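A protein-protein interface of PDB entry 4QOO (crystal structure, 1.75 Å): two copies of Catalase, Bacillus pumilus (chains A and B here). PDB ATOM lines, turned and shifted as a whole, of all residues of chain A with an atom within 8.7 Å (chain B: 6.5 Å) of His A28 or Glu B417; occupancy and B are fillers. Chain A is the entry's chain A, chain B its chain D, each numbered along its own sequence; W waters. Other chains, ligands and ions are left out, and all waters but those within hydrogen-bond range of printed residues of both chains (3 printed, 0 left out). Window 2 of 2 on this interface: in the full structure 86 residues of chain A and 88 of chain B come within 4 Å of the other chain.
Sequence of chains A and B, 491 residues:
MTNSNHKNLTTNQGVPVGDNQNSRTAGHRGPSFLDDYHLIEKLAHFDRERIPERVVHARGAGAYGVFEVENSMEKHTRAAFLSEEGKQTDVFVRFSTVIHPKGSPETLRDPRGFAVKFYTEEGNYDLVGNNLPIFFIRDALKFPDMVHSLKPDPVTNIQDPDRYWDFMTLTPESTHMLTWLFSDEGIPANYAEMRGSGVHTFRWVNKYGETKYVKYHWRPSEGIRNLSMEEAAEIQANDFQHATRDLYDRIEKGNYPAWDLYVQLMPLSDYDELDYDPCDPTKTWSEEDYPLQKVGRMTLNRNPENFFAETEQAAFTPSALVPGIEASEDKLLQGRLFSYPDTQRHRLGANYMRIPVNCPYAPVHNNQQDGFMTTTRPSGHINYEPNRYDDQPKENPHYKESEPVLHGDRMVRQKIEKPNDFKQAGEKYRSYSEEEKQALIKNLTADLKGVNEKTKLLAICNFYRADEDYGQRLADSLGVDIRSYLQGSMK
O of Gly A27 is in hydrogen-bond range of OG1 of Thr A25 (2.6 Å). O of Pro A31 is in hydrogen-bond range of N of Ala A26, at 3.0 Å. The side-chain amino group of Lys B418 is in hydrogen-bond range of the backbone carbonyl oxygen of Tyr B271 (2.8 Å). O of Gln B414 sits at hydrogen-bond distance from NZ of Lys B331 (2.7 Å).
Water W1 lies within hydrogen-bond range of O of Ser A23 (2.6 Å), NZ of Lys B331 (2.7 Å), OG1 of Thr A25 (2.8 Å) and N of Gln B414 (3.1 Å). Water W2 lies within hydrogen-bond range of the side-chain amide oxygen of Asn A22 and the side-chain amino group of Lys B331. Water W3 lies within hydrogen-bond range of the backbone carbonyl oxygen of Lys B331 (2.8 Å) and the side-chain hydroxyl of Ser A23 (2.9 Å).
Printed residues of chain B that touch a printed residue of chain A: Tyr B271, Asp B277, Lys B331, Gly B408, Arg B410, Val B412, Gln B414, Lys B415, Ile B416 and Glu B417. Hydrophobic or aromatic side chains of chain B within 4 Å of the printed part of chain A: Tyr B271, Val B412 and Ile B416. Hydrophobic or aromatic side chains of chain A within 4 Å of the printed part of chain B: His A28. Among the printed residues, 21 pairs touch across the chains. Among the printed residues, Asp or Glu carboxylates within 4 Å of a Lys or Arg side-chain nitrogen of the other chain: Arg A29 with Asp B277 (2.8 Å).
Gln B414 touches Asn A22 (N to CB, 3.5 Å). Lys B331 touches Thr A25 (NZ to OG1, 3.98 Å). O of Ala A26 touches CA of Gly B408, at 3.9 Å. C of Ala A26 touches O of Arg B410 (3.9 Å). CA of Gly B408 touches CA of Gly A27 (3.7 Å). C of Gly A27 touches CG2 of Val B412 (3.4 Å). Tyr B271 touches His A28 (OH to CE1, 3.9 Å). His A28 touches Gln B414 (CB to NE2, 3.5 Å). CB of His A28 touches O of Lys B415, 3.9 Å away. O of His A28 touches CG2 of Ile B416 (3.7 Å).
Of the printed residues of chain B, His A28 touches Tyr B271 (3.9 Å), Lys B331 (2.9 Å), Val B412 (3.9 Å), Gln B414 (3.5 Å), Lys B415 (3.9 Å), Ile B416 (3.7 Å) and Glu B417 (2.8 Å). Of the printed residues of chain A, Glu B417 touches His A28. Of chain A, only His A28 (3.7 Å) comes within 4 Å of Ile B416. Of the printed residues of chain B, Ser A23 touches Val B412. Of the printed residues of chain B, Arg A29 touches Tyr B271 and Asp B277. Of the printed residues of chain A, Asp B277 touches Arg A29. Of the printed residues of chain A, Arg B410 touches Thr A25, Ala A26 and Gly A27. Printed residues of chain A within 4 Å of Gln B414: Asn A22 (3.5 Å) and His A28 (3.5 Å). Tyr B276 touches none of the printed residues of chain A. Gly A30 touches none of the printed residues of chain B. The nearest printed residue of chain B that does not touch His A28 is Gly B408 (5.3 Å).
The side-chain amide oxygen (OD1) of Asn A22 is in hydrogen-bond range of the backbone NH (N) of Lys B415, 3.4 Å away. The backbone carbonyl oxygen of Val B412 is in hydrogen-bond range of the backbone NH of Thr A25. The backbone carbonyl oxygen of Arg B410 is in hydrogen-bond range of the backbone NH of Gly A27 (3.0 Å). The backbone carbonyl oxygen (O) of His A28 is in hydrogen-bond range of the side-chain amino group (NZ) of Lys B331 (2.9 Å). A ring nitrogen (NE2) of His A28 lies within hydrogen-bond range of the side-chain carboxylate of Glu B417. NH2 of Arg A29 lies within salt-bridge range of OD1 of Asp B277 (2.8 Å). O of Thr A25 lies close to O of Arg B410, at 3.5 Å.
No position is printed for both chains.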
ATOM      1  N   ASN A  22     -13.413  21.935 -27.665  1.00  0.00           N
ATOM      2  CA  ASN A  22     -12.647  22.737 -28.630  1.00  0.00           C
ATOM      3  C   ASN A  22     -12.774  22.219 -30.058  1.00  0.00           C
ATOM      4  O   ASN A  22     -12.600  20.985 -30.297  1.00  0.00           O
ATOM      5  CB  ASN A  22     -11.144  22.714 -28.283  1.00  0.00           C
ATOM      6  CG  ASN A  22     -10.874  23.160 -26.874  1.00  0.00           C
ATOM      7  OD1 ASN A  22     -11.137  24.336 -26.530  1.00  0.00           O
ATOM      8  ND2 ASN A  22     -10.443  22.229 -26.031  1.00  0.00           N
ATOM      9  N   SER A  23     -13.007  23.178 -30.976  1.00  0.00           N
ATOM     10  CA  SER A  23     -12.919  22.953 -32.406  1.00  0.00           C
ATOM     11  C   SER A  23     -11.471  22.651 -32.788  1.00  0.00           C
ATOM     12  O   SER A  23     -10.546  23.026 -32.068  1.00  0.00           O
ATOM     13  CB  SER A  23     -13.403  24.194 -33.170  1.00  0.00           C
ATOM     14  OG  SER A  23     -14.794  24.366 -32.890  1.00  0.00           O
ATOM     15  N   ARG A  24     -11.292  22.045 -33.945  1.00  0.00           N
ATOM     16  CA  ARG A  24      -9.951  21.780 -34.455  1.00  0.00           C
ATOM     17  C   ARG A  24      -9.435  22.910 -35.320  1.00  0.00           C
ATOM     18  O   ARG A  24     -10.123  23.298 -36.296  1.00  0.00           O
ATOM     19  CB  ARG A  24     -10.023  20.485 -35.256  1.00  0.00           C
ATOM     20  CG  ARG A  24      -8.736  19.784 -35.406  1.00  0.00           C
ATOM     21  CD  ARG A  24      -8.942  18.523 -36.214  1.00  0.00           C
ATOM     22  NE  ARG A  24      -7.747  17.678 -36.115  1.00  0.00           N
ATOM     23  CZ  ARG A  24      -7.474  16.701 -36.959  1.00  0.00           C
ATOM     24  NH1 ARG A  24      -8.300  16.443 -37.970  1.00  0.00           N
ATOM     25  NH2 ARG A  24      -6.405  15.962 -36.746  1.00  0.00           N
ATOM     26  N   THR A  25      -8.270  23.443 -34.994  1.00  0.00           N
ATOM     27  CA  THR A  25      -7.844  24.735 -35.471  1.00  0.00           C
ATOM     28  C   THR A  25      -6.358  24.736 -35.799  1.00  0.00           C
ATOM     29  O   THR A  25      -5.631  23.802 -35.408  1.00  0.00           O
ATOM     30  CB  THR A  25      -8.141  25.853 -34.423  1.00  0.00           C
ATOM     31  OG1 THR A  25      -7.442  25.573 -33.177  1.00  0.00           O
ATOM     32  CG2 THR A  25      -9.679  25.982 -34.160  1.00  0.00           C
ATOM     33  N   ALA A  26      -5.915  25.759 -36.533  1.00  0.00           N
ATOM     34  CA  ALA A  26      -4.496  26.015 -36.808  1.00  0.00           C
ATOM     35  C   ALA A  26      -3.813  26.647 -35.619  1.00  0.00           C
ATOM     36  O   ALA A  26      -3.806  27.875 -35.477  1.00  0.00           O
ATOM     37  CB  ALA A  26      -4.344  26.874 -38.045  1.00  0.00           C
ATOM     38  N   GLY A  27      -3.269  25.790 -34.753  1.00  0.00           N
ATOM     39  CA  GLY A  27      -2.817  26.221 -33.442  1.00  0.00           C
ATOM     40  C   GLY A  27      -3.930  26.668 -32.556  1.00  0.00           C
ATOM     41  O   GLY A  27      -5.120  26.605 -32.935  1.00  0.00           O
ATOM     42  N   HIS A  28      -3.572  27.176 -31.386  1.00  0.00           N
ATOM     43  CA  HIS A  28      -4.533  27.400 -30.314  1.00  0.00           C
ATOM     44  C   HIS A  28      -5.512  28.557 -30.611  1.00  0.00           C
ATOM     45  O   HIS A  28      -6.555  28.604 -30.009  1.00  0.00           O
ATOM     46  CB  HIS A  28      -3.764  27.659 -28.984  1.00  0.00           C
ATOM     47  CG  HIS A  28      -3.034  28.965 -28.962  1.00  0.00           C
ATOM     48  ND1 HIS A  28      -3.658  30.170 -28.686  1.00  0.00           N
ATOM     49  CD2 HIS A  28      -1.724  29.263 -29.171  1.00  0.00           C
ATOM     50  CE1 HIS A  28      -2.774  31.153 -28.755  1.00  0.00           C
ATOM     51  NE2 HIS A  28      -1.588  30.628 -29.030  1.00  0.00           N
ATOM     52  N   ARG A  29      -5.165  29.468 -31.522  1.00  0.00           N
ATOM     53  CA  ARG A  29      -6.041  30.573 -31.822  1.00  0.00           C
ATOM     54  C   ARG A  29      -6.389  30.749 -33.308  1.00  0.00           C
ATOM     55  O   ARG A  29      -7.002  31.779 -33.666  1.00  0.00           O
ATOM     56  CB  ARG A  29      -5.530  31.897 -31.235  1.00  0.00           C
ATOM     57  CG  ARG A  29      -4.238  32.363 -31.817  1.00  0.00           C
ATOM     58  CD  ARG A  29      -3.849  33.692 -31.249  1.00  0.00           C
ATOM     59  NE  ARG A  29      -4.971  34.642 -31.264  1.00  0.00           N
ATOM     60  CZ  ARG A  29      -5.405  35.340 -32.327  1.00  0.00           C
ATOM     61  NH1 ARG A  29      -4.829  35.236 -33.535  1.00  0.00           N
ATOM     62  NH2 ARG A  29      -6.462  36.179 -32.179  1.00  0.00           N
ATOM     63  N   GLY A  30      -6.080  29.753 -34.158  1.00  0.00           N
ATOM     64  CA  GLY A  30      -6.189  29.962 -35.603  1.00  0.00           C
ATOM     65  C   GLY A  30      -7.555  29.551 -36.093  1.00  0.00           C
ATOM     66  O   GLY A  30      -8.436  29.183 -35.283  1.00  0.00           O
ATOM     67  N   PRO A  31      -7.795  29.711 -37.420  1.00  0.00           N
ATOM     68  CA  PRO A  31      -9.063  29.379 -37.981  1.00  0.00           C
ATOM     69  C   PRO A  31      -9.315  27.874 -37.926  1.00  0.00           C
ATOM     70  O   PRO A  31      -8.375  27.070 -37.713  1.00  0.00           O
ATOM     71  CB  PRO A  31      -8.950  29.865 -39.446  1.00  0.00           C
ATOM     72  CG  PRO A  31      -7.519  30.015 -39.723  1.00  0.00           C
ATOM     73  CD  PRO A  31      -6.878  30.281 -38.411  1.00  0.00           C
ATOM     74  N   TYR B 271      -2.090  42.268 -30.560  1.00  0.00           N
ATOM     75  CA  TYR B 271      -2.347  41.031 -29.821  1.00  0.00           C
ATOM     76  C   TYR B 271      -1.499  40.925 -28.604  1.00  0.00           C
ATOM     77  O   TYR B 271      -1.995  40.672 -27.518  1.00  0.00           O
ATOM     78  CB  TYR B 271      -2.146  39.779 -30.706  1.00  0.00           C
ATOM     79  CG  TYR B 271      -2.278  38.475 -29.943  1.00  0.00           C
ATOM     80  CD1 TYR B 271      -3.517  37.850 -29.820  1.00  0.00           C
ATOM     81  CD2 TYR B 271      -1.163  37.861 -29.345  1.00  0.00           C
ATOM     82  CE1 TYR B 271      -3.668  36.660 -29.108  1.00  0.00           C
ATOM     83  CE2 TYR B 271      -1.305  36.685 -28.642  1.00  0.00           C
ATOM     84  CZ  TYR B 271      -2.581  36.107 -28.507  1.00  0.00           C
ATOM     85  OH  TYR B 271      -2.783  34.940 -27.815  1.00  0.00           O
ATOM     86  N   TYR B 276      -6.025  40.055 -23.046  1.00  0.00           N
ATOM     87  CA  TYR B 276      -7.019  39.140 -23.528  1.00  0.00           C
ATOM     88  C   TYR B 276      -6.740  38.933 -25.008  1.00  0.00           C
ATOM     89  O   TYR B 276      -5.896  39.618 -25.595  1.00  0.00           O
ATOM     90  CB  TYR B 276      -8.412  39.758 -23.247  1.00  0.00           C
ATOM     91  CG  TYR B 276      -8.643  41.110 -23.943  1.00  0.00           C
ATOM     92  CD1 TYR B 276      -8.280  42.292 -23.359  1.00  0.00           C
ATOM     93  CD2 TYR B 276      -9.242  41.175 -25.165  1.00  0.00           C
ATOM     94  CE1 TYR B 276      -8.485  43.516 -23.995  1.00  0.00           C
ATOM     95  CE2 TYR B 276      -9.436  42.354 -25.828  1.00  0.00           C
ATOM     96  CZ  TYR B 276      -9.038  43.534 -25.242  1.00  0.00           C
ATOM     97  OH  TYR B 276      -9.251  44.704 -25.911  1.00  0.00           O
ATOM     98  N   ASP B 277      -7.461  37.990 -25.613  1.00  0.00           N
ATOM     99  CA  ASP B 277      -7.370  37.746 -27.053  1.00  0.00           C
ATOM    100  C   ASP B 277      -8.392  38.644 -27.755  1.00  0.00           C
ATOM    101  O   ASP B 277      -9.591  38.549 -27.435  1.00  0.00           O
ATOM    102  CB  ASP B 277      -7.643  36.255 -27.308  1.00  0.00           C
ATOM    103  CG  ASP B 277      -7.445  35.862 -28.770  1.00  0.00           C
ATOM    104  OD1 ASP B 277      -7.719  36.707 -29.679  1.00  0.00           O
ATOM    105  OD2 ASP B 277      -7.004  34.715 -28.980  1.00  0.00           O
ATOM    106  N   ASP B 280     -11.544  36.953 -28.934  1.00  0.00           N
ATOM    107  CA  ASP B 280     -12.345  36.198 -27.987  1.00  0.00           C
ATOM    108  C   ASP B 280     -13.677  36.947 -27.905  1.00  0.00           C
ATOM    109  O   ASP B 280     -13.682  38.074 -27.395  1.00  0.00           O
ATOM    110  CB  ASP B 280     -11.632  36.223 -26.633  1.00  0.00           C
ATOM    111  CG  ASP B 280     -12.427  35.561 -25.511  1.00  0.00           C
ATOM    112  OD1 ASP B 280     -13.573  35.106 -25.742  1.00  0.00           O
ATOM    113  OD2 ASP B 280     -11.852  35.453 -24.380  1.00  0.00           O
ATOM    114  N   LYS B 331     -13.230  31.543 -32.921  1.00  0.00           N
ATOM    115  CA  LYS B 331     -13.627  30.135 -33.136  1.00  0.00           C
ATOM    116  C   LYS B 331     -15.153  30.002 -33.123  1.00  0.00           C
ATOM    117  O   LYS B 331     -15.717  29.006 -33.594  1.00  0.00           O
ATOM    118  CB  LYS B 331     -13.037  29.188 -32.057  1.00  0.00           C
ATOM    119  CG  LYS B 331     -11.528  29.088 -32.097  1.00  0.00           C
ATOM    120  CD  LYS B 331     -11.009  28.158 -31.040  1.00  0.00           C
ATOM    121  CE  LYS B 331      -9.491  28.304 -30.857  1.00  0.00           C
ATOM    122  NZ  LYS B 331      -9.088  27.208 -29.943  1.00  0.00           N
ATOM    123  N   GLY B 408      -0.045  28.976 -35.611  1.00  0.00           N
ATOM    124  CA  GLY B 408       0.073  27.579 -35.244  1.00  0.00           C
ATOM    125  C   GLY B 408       0.784  26.708 -36.256  1.00  0.00           C
ATOM    126  O   GLY B 408       0.692  26.896 -37.488  1.00  0.00           O
ATOM    127  N   ARG B 410       0.517  23.206 -35.808  1.00  0.00           N
ATOM    128  CA  ARG B 410      -0.189  21.904 -35.764  1.00  0.00           C
ATOM    129  C   ARG B 410      -1.730  22.086 -35.803  1.00  0.00           C
ATOM    130  O   ARG B 410      -2.252  23.054 -35.332  1.00  0.00           O
ATOM    131  CB  ARG B 410       0.166  21.149 -34.489  1.00  0.00           C
ATOM    132  CG  ARG B 410       1.587  20.586 -34.405  1.00  0.00           C
ATOM    133  CD  ARG B 410       1.784  20.034 -32.976  1.00  0.00           C
ATOM    134  NE  ARG B 410       1.897  18.578 -32.981  1.00  0.00           N
ATOM    135  CZ  ARG B 410       2.935  17.866 -33.432  1.00  0.00           C
ATOM    136  NH1 ARG B 410       2.879  16.543 -33.376  1.00  0.00           N
ATOM    137  NH2 ARG B 410       4.026  18.444 -33.923  1.00  0.00           N
ATOM    138  N   VAL B 412      -4.801  21.312 -33.873  1.00  0.00           N
ATOM    139  CA  VAL B 412      -4.998  21.055 -32.469  1.00  0.00           C
ATOM    140  C   VAL B 412      -6.449  21.299 -32.065  1.00  0.00           C
ATOM    141  O   VAL B 412      -7.153  22.120 -32.676  1.00  0.00           O
ATOM    142  CB  VAL B 412      -4.067  21.932 -31.566  1.00  0.00           C
ATOM    143  CG1 VAL B 412      -2.606  21.710 -31.932  1.00  0.00           C
ATOM    144  CG2 VAL B 412      -4.418  23.410 -31.568  1.00  0.00           C
ATOM    145  N   GLN B 414      -7.632  22.937 -28.699  1.00  0.00           N
ATOM    146  CA  GLN B 414      -6.991  23.542 -27.526  1.00  0.00           C
ATOM    147  C   GLN B 414      -7.596  24.892 -27.275  1.00  0.00           C
ATOM    148  O   GLN B 414      -7.769  25.675 -28.214  1.00  0.00           O
ATOM    149  CB  GLN B 414      -5.483  23.741 -27.825  1.00  0.00           C
ATOM    150  CG  GLN B 414      -4.624  24.138 -26.647  1.00  0.00           C
ATOM    151  CD  GLN B 414      -3.187  24.306 -27.138  1.00  0.00           C
ATOM    152  OE1 GLN B 414      -2.737  23.541 -28.012  1.00  0.00           O
ATOM    153  NE2 GLN B 414      -2.512  25.344 -26.670  1.00  0.00           N
ATOM    154  N   LYS B 415      -7.854  25.209 -26.004  1.00  0.00           N
ATOM    155  CA  LYS B 415      -8.428  26.536 -25.676  1.00  0.00           C
ATOM    156  C   LYS B 415      -7.430  27.640 -26.050  1.00  0.00           C
ATOM    157  O   LYS B 415      -6.205  27.441 -25.980  1.00  0.00           O
ATOM    158  CB  LYS B 415      -8.791  26.618 -24.165  1.00  0.00           C
ATOM    159  CG  LYS B 415      -9.566  27.863 -23.781  1.00  0.00           C
ATOM    160  CD  LYS B 415      -9.702  28.009 -22.271  1.00  0.00           C
ATOM    161  CE  LYS B 415     -10.612  26.960 -21.654  1.00  0.00           C
ATOM    162  NZ  LYS B 415     -10.607  27.181 -20.173  1.00  0.00           N
ATOM    163  N   ILE B 416      -7.931  28.816 -26.415  1.00  0.00           N
ATOM    164  CA  ILE B 416      -7.031  29.959 -26.593  1.00  0.00           C
ATOM    165  C   ILE B 416      -6.212  30.177 -25.335  1.00  0.00           C
ATOM    166  O   ILE B 416      -6.687  29.985 -24.167  1.00  0.00           O
ATOM    167  CB  ILE B 416      -7.840  31.286 -26.916  1.00  0.00           C
ATOM    168  CG1 ILE B 416      -8.886  31.558 -25.869  1.00  0.00           C
ATOM    169  CG2 ILE B 416      -8.526  31.225 -28.299  1.00  0.00           C
ATOM    170  CD1 ILE B 416      -9.408  33.009 -25.918  1.00  0.00           C
ATOM    171  N   GLU B 417      -5.018  30.723 -25.552  1.00  0.00           N
ATOM    172  CA  GLU B 417      -4.297  31.370 -24.459  1.00  0.00           C
ATOM    173  C   GLU B 417      -5.013  32.670 -24.003  1.00  0.00           C
ATOM    174  O   GLU B 417      -5.806  33.284 -24.731  1.00  0.00           O
ATOM    175  CB  GLU B 417      -2.859  31.708 -24.861  1.00  0.00           C
ATOM    176  CG  GLU B 417      -1.964  30.548 -25.193  1.00  0.00           C
ATOM    177  CD  GLU B 417      -0.793  31.024 -26.024  1.00  0.00           C
ATOM    178  OE1 GLU B 417      -0.576  32.254 -26.080  1.00  0.00           O
ATOM    179  OE2 GLU B 417      -0.132  30.189 -26.648  1.00  0.00           O
ATOM    180  N   LYS B 418      -4.704  33.081 -22.775  1.00  0.00           N
ATOM    181  CA  LYS B 418      -5.285  34.261 -22.105  1.00  0.00           C
ATOM    182  C   LYS B 418      -6.836  34.319 -22.183  1.00  0.00           C
ATOM    183  O   LYS B 418      -7.397  35.349 -22.551  1.00  0.00           O
ATOM    184  CB  LYS B 418      -4.654  35.585 -22.458  1.00  0.00           C
ATOM    185  CG  LYS B 418      -4.324  35.829 -23.906  1.00  0.00           C
ATOM    186  CD  LYS B 418      -3.432  37.059 -24.042  1.00  0.00           C
ATOM    187  CE  LYS B 418      -3.371  37.359 -25.489  1.00  0.00           C
ATOM    188  NZ  LYS B 418      -2.800  38.685 -25.722  1.00  0.00           N
ATOM    189  N   PRO B 419      -7.482  33.215 -21.783  1.00  0.00           N
ATOM    190  CA  PRO B 419      -8.924  33.245 -21.656  1.00  0.00           C
ATOM    191  C   PRO B 419      -9.428  34.375 -20.751  1.00  0.00           C
ATOM    192  O   PRO B 419     -10.440  35.031 -21.091  1.00  0.00           O
ATOM    193  CB  PRO B 419      -9.260  31.886 -21.075  1.00  0.00           C
ATOM    194  CG  PRO B 419      -7.978  31.402 -20.442  1.00  0.00           C
ATOM    195  CD  PRO B 419      -6.891  31.982 -21.248  1.00  0.00           C
ATOM    196  N   ASN B 420      -8.709  34.668 -19.668  1.00  0.00           N
ATOM    197  CA  ASN B 420      -9.058  35.803 -18.778  1.00  0.00           C
ATOM    198  C   ASN B 420     -10.590  35.926 -18.546  1.00  0.00           C
ATOM    199  O   ASN B 420     -11.207  36.950 -18.896  1.00  0.00           O
ATOM    200  CB  ASN B 420      -8.577  37.137 -19.373  1.00  0.00           C
ATOM    201  CG  ASN B 420      -8.174  38.110 -18.291  1.00  0.00           C
ATOM    202  OD1 ASN B 420      -8.621  37.910 -17.163  1.00  0.00           O
ATOM    203  ND2 ASN B 420      -7.279  39.085 -18.568  1.00  0.00           N
HETATM  204  O   HOH W   1      -8.873  24.692 -30.988  1.00  0.00           O
HETATM  205  O   HOH W   2     -11.509  26.350 -28.128  1.00  0.00           O
HETATM  206  O   HOH W   3     -15.158  26.496 -34.802  1.00  0.00           O
